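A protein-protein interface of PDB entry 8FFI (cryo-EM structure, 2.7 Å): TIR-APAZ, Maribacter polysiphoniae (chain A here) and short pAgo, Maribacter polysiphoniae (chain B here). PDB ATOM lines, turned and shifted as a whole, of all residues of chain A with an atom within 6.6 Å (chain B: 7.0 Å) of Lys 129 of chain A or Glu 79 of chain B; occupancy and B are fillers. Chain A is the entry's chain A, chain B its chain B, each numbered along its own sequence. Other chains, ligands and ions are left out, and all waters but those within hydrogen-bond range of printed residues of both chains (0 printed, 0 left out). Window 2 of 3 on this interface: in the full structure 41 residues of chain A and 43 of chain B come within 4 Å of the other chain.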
ATOM      1  N   PHE A 120     -17.937  25.036 -26.561  1.00  0.00           N
ATOM      2  CA  PHE A 120     -16.520  25.138 -26.877  1.00  0.00           C
ATOM      3  C   PHE A 120     -15.960  26.545 -26.748  1.00  0.00           C
ATOM      4  O   PHE A 120     -14.752  26.722 -26.929  1.00  0.00           O
ATOM      5  CB  PHE A 120     -16.252  24.651 -28.309  1.00  0.00           C
ATOM      6  CG  PHE A 120     -15.950  23.188 -28.415  1.00  0.00           C
ATOM      7  CD1 PHE A 120     -16.967  22.271 -28.609  1.00  0.00           C
ATOM      8  CD2 PHE A 120     -14.648  22.732 -28.340  1.00  0.00           C
ATOM      9  CE1 PHE A 120     -16.689  20.926 -28.714  1.00  0.00           C
ATOM     10  CE2 PHE A 120     -14.365  21.389 -28.447  1.00  0.00           C
ATOM     11  CZ  PHE A 120     -15.386  20.486 -28.633  1.00  0.00           C
ATOM     12  N   SER A 123     -13.293  27.312 -23.785  1.00  0.00           N
ATOM     13  CA  SER A 123     -12.099  26.485 -23.896  1.00  0.00           C
ATOM     14  C   SER A 123     -12.427  25.267 -24.742  1.00  0.00           C
ATOM     15  O   SER A 123     -13.564  24.783 -24.737  1.00  0.00           O
ATOM     16  CB  SER A 123     -11.579  26.054 -22.520  1.00  0.00           C
ATOM     17  OG  SER A 123     -12.547  25.288 -21.828  1.00  0.00           O
ATOM     18  N   TRP A 124     -11.421  24.776 -25.466  1.00  0.00           N
ATOM     19  CA  TRP A 124     -11.596  23.615 -26.329  1.00  0.00           C
ATOM     20  C   TRP A 124     -11.279  22.298 -25.632  1.00  0.00           C
ATOM     21  O   TRP A 124     -11.792  21.254 -26.052  1.00  0.00           O
ATOM     22  CB  TRP A 124     -10.724  23.751 -27.581  1.00  0.00           C
ATOM     23  CG  TRP A 124     -11.223  24.775 -28.564  1.00  0.00           C
ATOM     24  CD1 TRP A 124     -12.343  25.542 -28.449  1.00  0.00           C
ATOM     25  CD2 TRP A 124     -10.616  25.137 -29.812  1.00  0.00           C
ATOM     26  NE1 TRP A 124     -12.474  26.361 -29.542  1.00  0.00           N
ATOM     27  CE2 TRP A 124     -11.426  26.129 -30.396  1.00  0.00           C
ATOM     28  CE3 TRP A 124      -9.469  24.720 -30.491  1.00  0.00           C
ATOM     29  CZ2 TRP A 124     -11.124  26.712 -31.627  1.00  0.00           C
ATOM     30  CZ3 TRP A 124      -9.171  25.298 -31.713  1.00  0.00           C
ATOM     31  CH2 TRP A 124      -9.995  26.284 -32.267  1.00  0.00           C
ATOM     32  N   ALA A 125     -10.450  22.321 -24.585  1.00  0.00           N
ATOM     33  CA  ALA A 125     -10.097  21.088 -23.887  1.00  0.00           C
ATOM     34  C   ALA A 125     -11.311  20.471 -23.204  1.00  0.00           C
ATOM     35  O   ALA A 125     -11.545  19.259 -23.302  1.00  0.00           O
ATOM     36  CB  ALA A 125      -8.990  21.362 -22.870  1.00  0.00           C
ATOM     37  N   ARG A 126     -12.103  21.291 -22.507  1.00  0.00           N
ATOM     38  CA  ARG A 126     -13.280  20.751 -21.838  1.00  0.00           C
ATOM     39  C   ARG A 126     -14.358  20.357 -22.839  1.00  0.00           C
ATOM     40  O   ARG A 126     -15.118  19.418 -22.585  1.00  0.00           O
ATOM     41  CB  ARG A 126     -13.820  21.749 -20.812  1.00  0.00           C
ATOM     42  CG  ARG A 126     -14.663  22.875 -21.377  1.00  0.00           C
ATOM     43  CD  ARG A 126     -15.050  23.854 -20.281  1.00  0.00           C
ATOM     44  NE  ARG A 126     -13.899  24.594 -19.777  1.00  0.00           N
ATOM     45  CZ  ARG A 126     -13.940  25.442 -18.759  1.00  0.00           C
ATOM     46  NH1 ARG A 126     -15.065  25.683 -18.105  1.00  0.00           N
ATOM     47  NH2 ARG A 126     -12.826  26.065 -18.387  1.00  0.00           N
ATOM     48  N   GLY A 127     -14.426  21.036 -23.986  1.00  0.00           N
ATOM     49  CA  GLY A 127     -15.321  20.585 -25.040  1.00  0.00           C
ATOM     50  C   GLY A 127     -14.931  19.223 -25.584  1.00  0.00           C
ATOM     51  O   GLY A 127     -15.789  18.366 -25.819  1.00  0.00           O
ATOM     52  N   LEU A 128     -13.630  19.005 -25.794  1.00  0.00           N
ATOM     53  CA  LEU A 128     -13.160  17.695 -26.232  1.00  0.00           C
ATOM     54  C   LEU A 128     -13.458  16.628 -25.187  1.00  0.00           C
ATOM     55  O   LEU A 128     -13.866  15.510 -25.526  1.00  0.00           O
ATOM     56  CB  LEU A 128     -11.663  17.753 -26.536  1.00  0.00           C
ATOM     57  CG  LEU A 128     -11.094  16.641 -27.418  1.00  0.00           C
ATOM     58  CD1 LEU A 128     -11.750  16.650 -28.787  1.00  0.00           C
ATOM     59  CD2 LEU A 128      -9.587  16.779 -27.544  1.00  0.00           C
ATOM     60  N   LYS A 129     -13.259  16.956 -23.908  1.00  0.00           N
ATOM     61  CA  LYS A 129     -13.587  16.011 -22.845  1.00  0.00           C
ATOM     62  C   LYS A 129     -15.076  15.690 -22.830  1.00  0.00           C
ATOM     63  O   LYS A 129     -15.466  14.534 -22.630  1.00  0.00           O
ATOM     64  CB  LYS A 129     -13.146  16.564 -21.490  1.00  0.00           C
ATOM     65  CG  LYS A 129     -11.649  16.527 -21.269  1.00  0.00           C
ATOM     66  CD  LYS A 129     -11.279  17.059 -19.896  1.00  0.00           C
ATOM     67  CE  LYS A 129      -9.778  16.987 -19.671  1.00  0.00           C
ATOM     68  NZ  LYS A 129      -9.035  17.860 -20.621  1.00  0.00           N
ATOM     69  N   ASP A 130     -15.924  16.700 -23.036  1.00  0.00           N
ATOM     70  CA  ASP A 130     -17.363  16.464 -23.089  1.00  0.00           C
ATOM     71  C   ASP A 130     -17.733  15.563 -24.259  1.00  0.00           C
ATOM     72  O   ASP A 130     -18.571  14.666 -24.119  1.00  0.00           O
ATOM     73  CB  ASP A 130     -18.111  17.794 -23.182  1.00  0.00           C
ATOM     74  CG  ASP A 130     -18.292  18.456 -21.833  1.00  0.00           C
ATOM     75  OD1 ASP A 130     -18.346  17.734 -20.815  1.00  0.00           O
ATOM     76  OD2 ASP A 130     -18.384  19.701 -21.791  1.00  0.00           O
ATOM     77  N   ILE A 131     -17.123  15.791 -25.426  1.00  0.00           N
ATOM     78  CA  ILE A 131     -17.395  14.936 -26.581  1.00  0.00           C
ATOM     79  C   ILE A 131     -16.981  13.499 -26.289  1.00  0.00           C
ATOM     80  O   ILE A 131     -17.714  12.550 -26.600  1.00  0.00           O
ATOM     81  CB  ILE A 131     -16.689  15.477 -27.839  1.00  0.00           C
ATOM     82  CG1 ILE A 131     -17.239  16.847 -28.226  1.00  0.00           C
ATOM     83  CG2 ILE A 131     -16.849  14.507 -28.999  1.00  0.00           C
ATOM     84  CD1 ILE A 131     -16.637  17.394 -29.496  1.00  0.00           C
ATOM     85  N   LEU A 132     -15.800  13.315 -25.695  1.00  0.00           N
ATOM     86  CA  LEU A 132     -15.336  11.968 -25.380  1.00  0.00           C
ATOM     87  C   LEU A 132     -16.256  11.281 -24.378  1.00  0.00           C
ATOM     88  O   LEU A 132     -16.581  10.097 -24.532  1.00  0.00           O
ATOM     89  CB  LEU A 132     -13.902  12.017 -24.850  1.00  0.00           C
ATOM     90  CG  LEU A 132     -12.792  11.737 -25.865  1.00  0.00           C
ATOM     91  CD1 LEU A 132     -12.648  12.880 -26.855  1.00  0.00           C
ATOM     92  CD2 LEU A 132     -11.473  11.472 -25.155  1.00  0.00           C
ATOM     93  N   GLU A 133     -16.690  12.008 -23.346  1.00  0.00           N
ATOM     94  CA  GLU A 133     -17.591  11.423 -22.357  1.00  0.00           C
ATOM     95  C   GLU A 133     -18.934  11.059 -22.979  1.00  0.00           C
ATOM     96  O   GLU A 133     -19.498  10.003 -22.677  1.00  0.00           O
ATOM     97  CB  GLU A 133     -17.783  12.386 -21.185  1.00  0.00           C
ATOM     98  CG  GLU A 133     -16.551  12.550 -20.313  1.00  0.00           C
ATOM     99  CD  GLU A 133     -16.164  11.269 -19.600  1.00  0.00           C
ATOM    100  OE1 GLU A 133     -17.071  10.493 -19.232  1.00  0.00           O
ATOM    101  OE2 GLU A 133     -14.952  11.036 -19.409  1.00  0.00           O
ATOM    102  N   ALA A 134     -19.462  11.923 -23.851  1.00  0.00           N
ATOM    103  CA  ALA A 134     -20.715  11.611 -24.530  1.00  0.00           C
ATOM    104  C   ALA A 134     -20.576  10.372 -25.403  1.00  0.00           C
ATOM    105  O   ALA A 134     -21.466   9.513 -25.423  1.00  0.00           O
ATOM    106  CB  ALA A 134     -21.171  12.806 -25.367  1.00  0.00           C
ATOM    107  N   GLU A 136     -18.431   7.895 -25.022  1.00  0.00           N
ATOM    108  CA  GLU A 136     -18.314   6.725 -24.156  1.00  0.00           C
ATOM    109  C   GLU A 136     -19.660   6.347 -23.551  1.00  0.00           C
ATOM    110  O   GLU A 136     -19.951   5.160 -23.363  1.00  0.00           O
ATOM    111  CB  GLU A 136     -17.285   6.981 -23.056  1.00  0.00           C
ATOM    112  CG  GLU A 136     -15.862   7.148 -23.557  1.00  0.00           C
ATOM    113  CD  GLU A 136     -15.035   8.047 -22.659  1.00  0.00           C
ATOM    114  OE1 GLU A 136     -15.222   7.990 -21.425  1.00  0.00           O
ATOM    115  OE2 GLU A 136     -14.197   8.809 -23.186  1.00  0.00           O
ATOM    116  N   ILE B  60      -5.906  33.902 -22.716  1.00  0.00           N
ATOM    117  CA  ILE B  60      -5.258  32.784 -23.393  1.00  0.00           C
ATOM    118  C   ILE B  60      -5.870  31.442 -22.985  1.00  0.00           C
ATOM    119  O   ILE B  60      -5.269  30.394 -23.217  1.00  0.00           O
ATOM    120  CB  ILE B  60      -3.738  32.786 -23.172  1.00  0.00           C
ATOM    121  CG1 ILE B  60      -3.402  32.530 -21.702  1.00  0.00           C
ATOM    122  CG2 ILE B  60      -3.136  34.097 -23.642  1.00  0.00           C
ATOM    123  CD1 ILE B  60      -1.946  32.230 -21.458  1.00  0.00           C
ATOM    124  N   GLN B  61      -7.054  31.456 -22.377  1.00  0.00           N
ATOM    125  CA  GLN B  61      -7.794  30.220 -22.164  1.00  0.00           C
ATOM    126  C   GLN B  61      -8.634  29.840 -23.373  1.00  0.00           C
ATOM    127  O   GLN B  61      -9.192  28.739 -23.403  1.00  0.00           O
ATOM    128  CB  GLN B  61      -8.694  30.345 -20.932  1.00  0.00           C
ATOM    129  CG  GLN B  61      -8.018  30.956 -19.717  1.00  0.00           C
ATOM    130  CD  GLN B  61      -7.065  29.998 -19.032  1.00  0.00           C
ATOM    131  OE1 GLN B  61      -7.322  28.799 -18.953  1.00  0.00           O
ATOM    132  NE2 GLN B  61      -5.958  30.526 -18.529  1.00  0.00           N
ATOM    133  N   PHE B  75      -3.207  29.377 -32.062  1.00  0.00           N
ATOM    134  CA  PHE B  75      -3.144  28.921 -30.682  1.00  0.00           C
ATOM    135  C   PHE B  75      -4.515  28.422 -30.253  1.00  0.00           C
ATOM    136  O   PHE B  75      -5.450  29.230 -30.155  1.00  0.00           O
ATOM    137  CB  PHE B  75      -2.681  30.059 -29.773  1.00  0.00           C
ATOM    138  CG  PHE B  75      -2.336  29.628 -28.380  1.00  0.00           C
ATOM    139  CD1 PHE B  75      -1.343  28.692 -28.156  1.00  0.00           C
ATOM    140  CD2 PHE B  75      -2.999  30.165 -27.292  1.00  0.00           C
ATOM    141  CE1 PHE B  75      -1.023  28.297 -26.876  1.00  0.00           C
ATOM    142  CE2 PHE B  75      -2.681  29.774 -26.008  1.00  0.00           C
ATOM    143  CZ  PHE B  75      -1.693  28.839 -25.800  1.00  0.00           C
ATOM    144  N   PRO B  76      -4.690  27.130 -29.987  1.00  0.00           N
ATOM    145  CA  PRO B  76      -6.006  26.607 -29.588  1.00  0.00           C
ATOM    146  C   PRO B  76      -6.322  26.683 -28.099  1.00  0.00           C
ATOM    147  O   PRO B  76      -7.270  26.023 -27.664  1.00  0.00           O
ATOM    148  CB  PRO B  76      -5.931  25.139 -30.036  1.00  0.00           C
ATOM    149  CG  PRO B  76      -4.482  24.811 -30.128  1.00  0.00           C
ATOM    150  CD  PRO B  76      -3.675  26.070 -30.100  1.00  0.00           C
ATOM    151  N   GLY B  77      -5.579  27.444 -27.315  1.00  0.00           N
ATOM    152  CA  GLY B  77      -5.839  27.543 -25.894  1.00  0.00           C
ATOM    153  C   GLY B  77      -4.795  26.798 -25.080  1.00  0.00           C
ATOM    154  O   GLY B  77      -4.237  25.781 -25.512  1.00  0.00           O
ATOM    155  N   PHE B  78      -4.526  27.312 -23.877  1.00  0.00           N
ATOM    156  CA  PHE B  78      -3.452  26.754 -23.061  1.00  0.00           C
ATOM    157  C   PHE B  78      -3.759  25.325 -22.626  1.00  0.00           C
ATOM    158  O   PHE B  78      -2.881  24.454 -22.671  1.00  0.00           O
ATOM    159  CB  PHE B  78      -3.197  27.643 -21.843  1.00  0.00           C
ATOM    160  CG  PHE B  78      -1.965  27.268 -21.070  1.00  0.00           C
ATOM    161  CD1 PHE B  78      -0.737  27.819 -21.390  1.00  0.00           C
ATOM    162  CD2 PHE B  78      -2.034  26.362 -20.027  1.00  0.00           C
ATOM    163  CE1 PHE B  78       0.397  27.473 -20.685  1.00  0.00           C
ATOM    164  CE2 PHE B  78      -0.903  26.009 -19.324  1.00  0.00           C
ATOM    165  CZ  PHE B  78       0.314  26.568 -19.651  1.00  0.00           C
ATOM    166  N   GLU B  79      -4.994  25.063 -22.197  1.00  0.00           N
ATOM    167  CA  GLU B  79      -5.329  23.726 -21.720  1.00  0.00           C
ATOM    168  C   GLU B  79      -5.466  22.739 -22.871  1.00  0.00           C
ATOM    169  O   GLU B  79      -5.219  21.541 -22.692  1.00  0.00           O
ATOM    170  CB  GLU B  79      -6.613  23.767 -20.894  1.00  0.00           C
ATOM    171  CG  GLU B  79      -6.744  22.635 -19.889  1.00  0.00           C
ATOM    172  CD  GLU B  79      -8.143  22.520 -19.319  1.00  0.00           C
ATOM    173  OE1 GLU B  79      -8.672  23.538 -18.828  1.00  0.00           O
ATOM    174  OE2 GLU B  79      -8.716  21.412 -19.366  1.00  0.00           O
ATOM    175  N   ALA B  80      -5.864  23.217 -24.051  1.00  0.00           N
ATOM    176  CA  ALA B  80      -5.903  22.348 -25.222  1.00  0.00           C
ATOM    177  C   ALA B  80      -4.506  21.889 -25.611  1.00  0.00           C
ATOM    178  O   ALA B  80      -4.308  20.730 -25.996  1.00  0.00           O
ATOM    179  CB  ALA B  80      -6.580  23.067 -26.388  1.00  0.00           C
ATOM    180  N   VAL B  81      -3.521  22.780 -25.514  1.00  0.00           N
ATOM    181  CA  VAL B  81      -2.157  22.439 -25.911  1.00  0.00           C
ATOM    182  C   VAL B  81      -1.464  21.622 -24.829  1.00  0.00           C
ATOM    183  O   VAL B  81      -1.067  20.473 -25.053  1.00  0.00           O
ATOM    184  CB  VAL B  81      -1.356  23.712 -26.240  1.00  0.00           C
ATOM    185  CG1 VAL B  81       0.063  23.348 -26.644  1.00  0.00           C
ATOM    186  CG2 VAL B  81      -2.032  24.496 -27.343  1.00  0.00           C
ATOM    187  N   PHE B  82      -1.309  22.199 -23.640  1.00  0.00           N
ATOM    188  CA  PHE B  82      -0.385  21.667 -22.649  1.00  0.00           C
ATOM    189  C   PHE B  82      -1.029  20.709 -21.657  1.00  0.00           C
ATOM    190  O   PHE B  82      -0.315  20.140 -20.827  1.00  0.00           O
ATOM    191  CB  PHE B  82       0.285  22.821 -21.901  1.00  0.00           C
ATOM    192  CG  PHE B  82       1.230  23.617 -22.752  1.00  0.00           C
ATOM    193  CD1 PHE B  82       2.400  23.052 -23.228  1.00  0.00           C
ATOM    194  CD2 PHE B  82       0.944  24.927 -23.090  1.00  0.00           C
ATOM    195  CE1 PHE B  82       3.266  23.779 -24.018  1.00  0.00           C
ATOM    196  CE2 PHE B  82       1.809  25.658 -23.879  1.00  0.00           C
ATOM    197  CZ  PHE B  82       2.973  25.083 -24.340  1.00  0.00           C
ATOM    198  N   ASP B  83      -2.346  20.510 -21.728  1.00  0.00           N
ATOM    199  CA  ASP B  83      -3.050  19.562 -20.861  1.00  0.00           C
ATOM    200  C   ASP B  83      -2.769  19.834 -19.385  1.00  0.00           C
ATOM    201  O   ASP B  83      -2.545  18.919 -18.590  1.00  0.00           O
ATOM    202  CB  ASP B  83      -2.697  18.120 -21.229  1.00  0.00           C
ATOM    203  CG  ASP B  83      -3.218  17.724 -22.596  1.00  0.00           C
ATOM    204  OD1 ASP B  83      -2.502  17.941 -23.596  1.00  0.00           O
ATOM    205  OD2 ASP B  83      -4.343  17.190 -22.671  1.00  0.00           O
ATOM    206  N   CYS B  84      -2.783  21.113 -19.015  1.00  0.00           N
ATOM    207  CA  CYS B  84      -2.586  21.517 -17.633  1.00  0.00           C
ATOM    208  C   CYS B  84      -3.276  22.854 -17.418  1.00  0.00           C
ATOM    209  O   CYS B  84      -3.630  23.552 -18.371  1.00  0.00           O
ATOM    210  CB  CYS B  84      -1.097  21.605 -17.268  1.00  0.00           C
ATOM    211  SG  CYS B  84      -0.167  22.867 -18.151  1.00  0.00           S
ATOM    212  N   LYS B  85      -3.463  23.203 -16.149  1.00  0.00           N
ATOM    213  CA  LYS B  85      -4.249  24.366 -15.764  1.00  0.00           C
ATOM    214  C   LYS B  85      -3.324  25.521 -15.407  1.00  0.00           C
ATOM    215  O   LYS B  85      -2.467  25.387 -14.529  1.00  0.00           O
ATOM    216  CB  LYS B  85      -5.159  24.027 -14.583  1.00  0.00           C
ATOM    217  CG  LYS B  85      -6.196  22.967 -14.889  1.00  0.00           C
ATOM    218  CD  LYS B  85      -7.109  22.728 -13.701  1.00  0.00           C
ATOM    219  CE  LYS B  85      -8.298  21.866 -14.085  1.00  0.00           C
ATOM    220  NZ  LYS B  85      -7.892  20.463 -14.374  1.00  0.00           N
ATOM    221  N   TRP B  86      -3.501  26.653 -16.086  1.00  0.00           N
ATOM    222  CA  TRP B  86      -2.801  27.895 -15.752  1.00  0.00           C
ATOM    223  C   TRP B  86      -3.841  29.006 -15.870  1.00  0.00           C
ATOM    224  O   TRP B  86      -4.004  29.609 -16.934  1.00  0.00           O
ATOM    225  CB  TRP B  86      -1.604  28.127 -16.664  1.00  0.00           C
ATOM    226  CG  TRP B  86      -0.807  29.348 -16.332  1.00  0.00           C
ATOM    227  CD1 TRP B  86      -0.560  29.850 -15.091  1.00  0.00           C
ATOM    228  CD2 TRP B  86      -0.146  30.219 -17.257  1.00  0.00           C
ATOM    229  NE1 TRP B  86       0.211  30.981 -15.183  1.00  0.00           N
ATOM    230  CE2 TRP B  86       0.479  31.231 -16.503  1.00  0.00           C
ATOM    231  CE3 TRP B  86      -0.027  30.247 -18.649  1.00  0.00           C
ATOM    232  CZ2 TRP B  86       1.212  32.257 -17.094  1.00  0.00           C
ATOM    233  CZ3 TRP B  86       0.705  31.265 -19.233  1.00  0.00           C
ATOM    234  CH2 TRP B  86       1.315  32.255 -18.456  1.00  0.00           C
ATOM    235  N   GLU B  87      -4.538  29.275 -14.769  1.00  0.00           N
ATOM    236  CA  GLU B  87      -5.668  30.191 -14.762  1.00  0.00           C
ATOM    237  C   GLU B  87      -5.509  31.199 -13.633  1.00  0.00           C
ATOM    238  O   GLU B  87      -4.805  30.961 -12.650  1.00  0.00           O
ATOM    239  CB  GLU B  87      -7.004  29.445 -14.620  1.00  0.00           C
ATOM    240  CG  GLU B  87      -7.176  28.658 -13.327  1.00  0.00           C
ATOM    241  CD  GLU B  87      -6.418  27.340 -13.315  1.00  0.00           C
ATOM    242  OE1 GLU B  87      -5.196  27.337 -13.572  1.00  0.00           O
ATOM    243  OE2 GLU B  87      -7.053  26.299 -13.041  1.00  0.00           O
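The side-chain amino group (NZ) of Lys 129 of chain A lies within salt-bridge range of the side-chain carboxylate (OE2) of Glu 79 of chain B.
Printed residues of chain B within 4 Å of Ser 123 of chain A: Gln 61.
Printed residues of chain B within 4 Å of Trp 124 of chain A: Pro 76.
Of the printed residues of chain B, Ala 125 of chain A touches Glu 79 and Ala 80.
Lys 129 of chain A touches just one residue of chain B: Glu 79 (3.8 Å).
Ile 131 of chain A touches none of the printed residues of chain B.
Of the printed residues of chain A, Pro 76 of chain B touches Trp 124.
Glu 79 of chain B touches two residues of chain A.
The nearest residue of chain B that does not touch Lys 129 of chain A is Asp 83 of chain B (5.2 Å).
The nearest residue of chain A that does not touch Glu 79 of chain B is Arg 126 of chain A (4.6 Å).
Among the printed residues, pairs that only touch across the chains: Ser 123 of chain A with Gln 61 of chain B (3.7 Å), Trp 124 of chain A with Pro 76 of chain B (3.6 Å), Ala 125 of chain A with Glu 79 of chain B (3.5 Å) and Ala 125 of chain A with Ala 80 of chain B (3.8 Å).
Printed residues of chain A that touch a printed residue of chain B: Ser 123, Trp 124, Ala 125 and Lys 129.
Hydrophobic or aromatic side chains of chain A that line the printed part of chain B: Trp 124 and Ala 125.
Among the printed residues, Asp or Glu carboxylates within 4 Å of a Lys or Arg side-chain nitrogen of the other chain: Lys 129 of chain A with Glu 79 of chain B (3.8 Å).
O of Phe 120 of chain A sits close to NE1 of Trp 124 of chain A, 3.5 Å away.
The guanidinium group (NE) of Arg 126 of chain A is in hydrogen-bond range of the side-chain hydroxyl (OG) of Ser 123 of chain A, 2.6 Å away.
O of Trp 86 of chain B is in hydrogen-bond range of NE2 of Gln 61 of chain B, 2.7 Å away.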
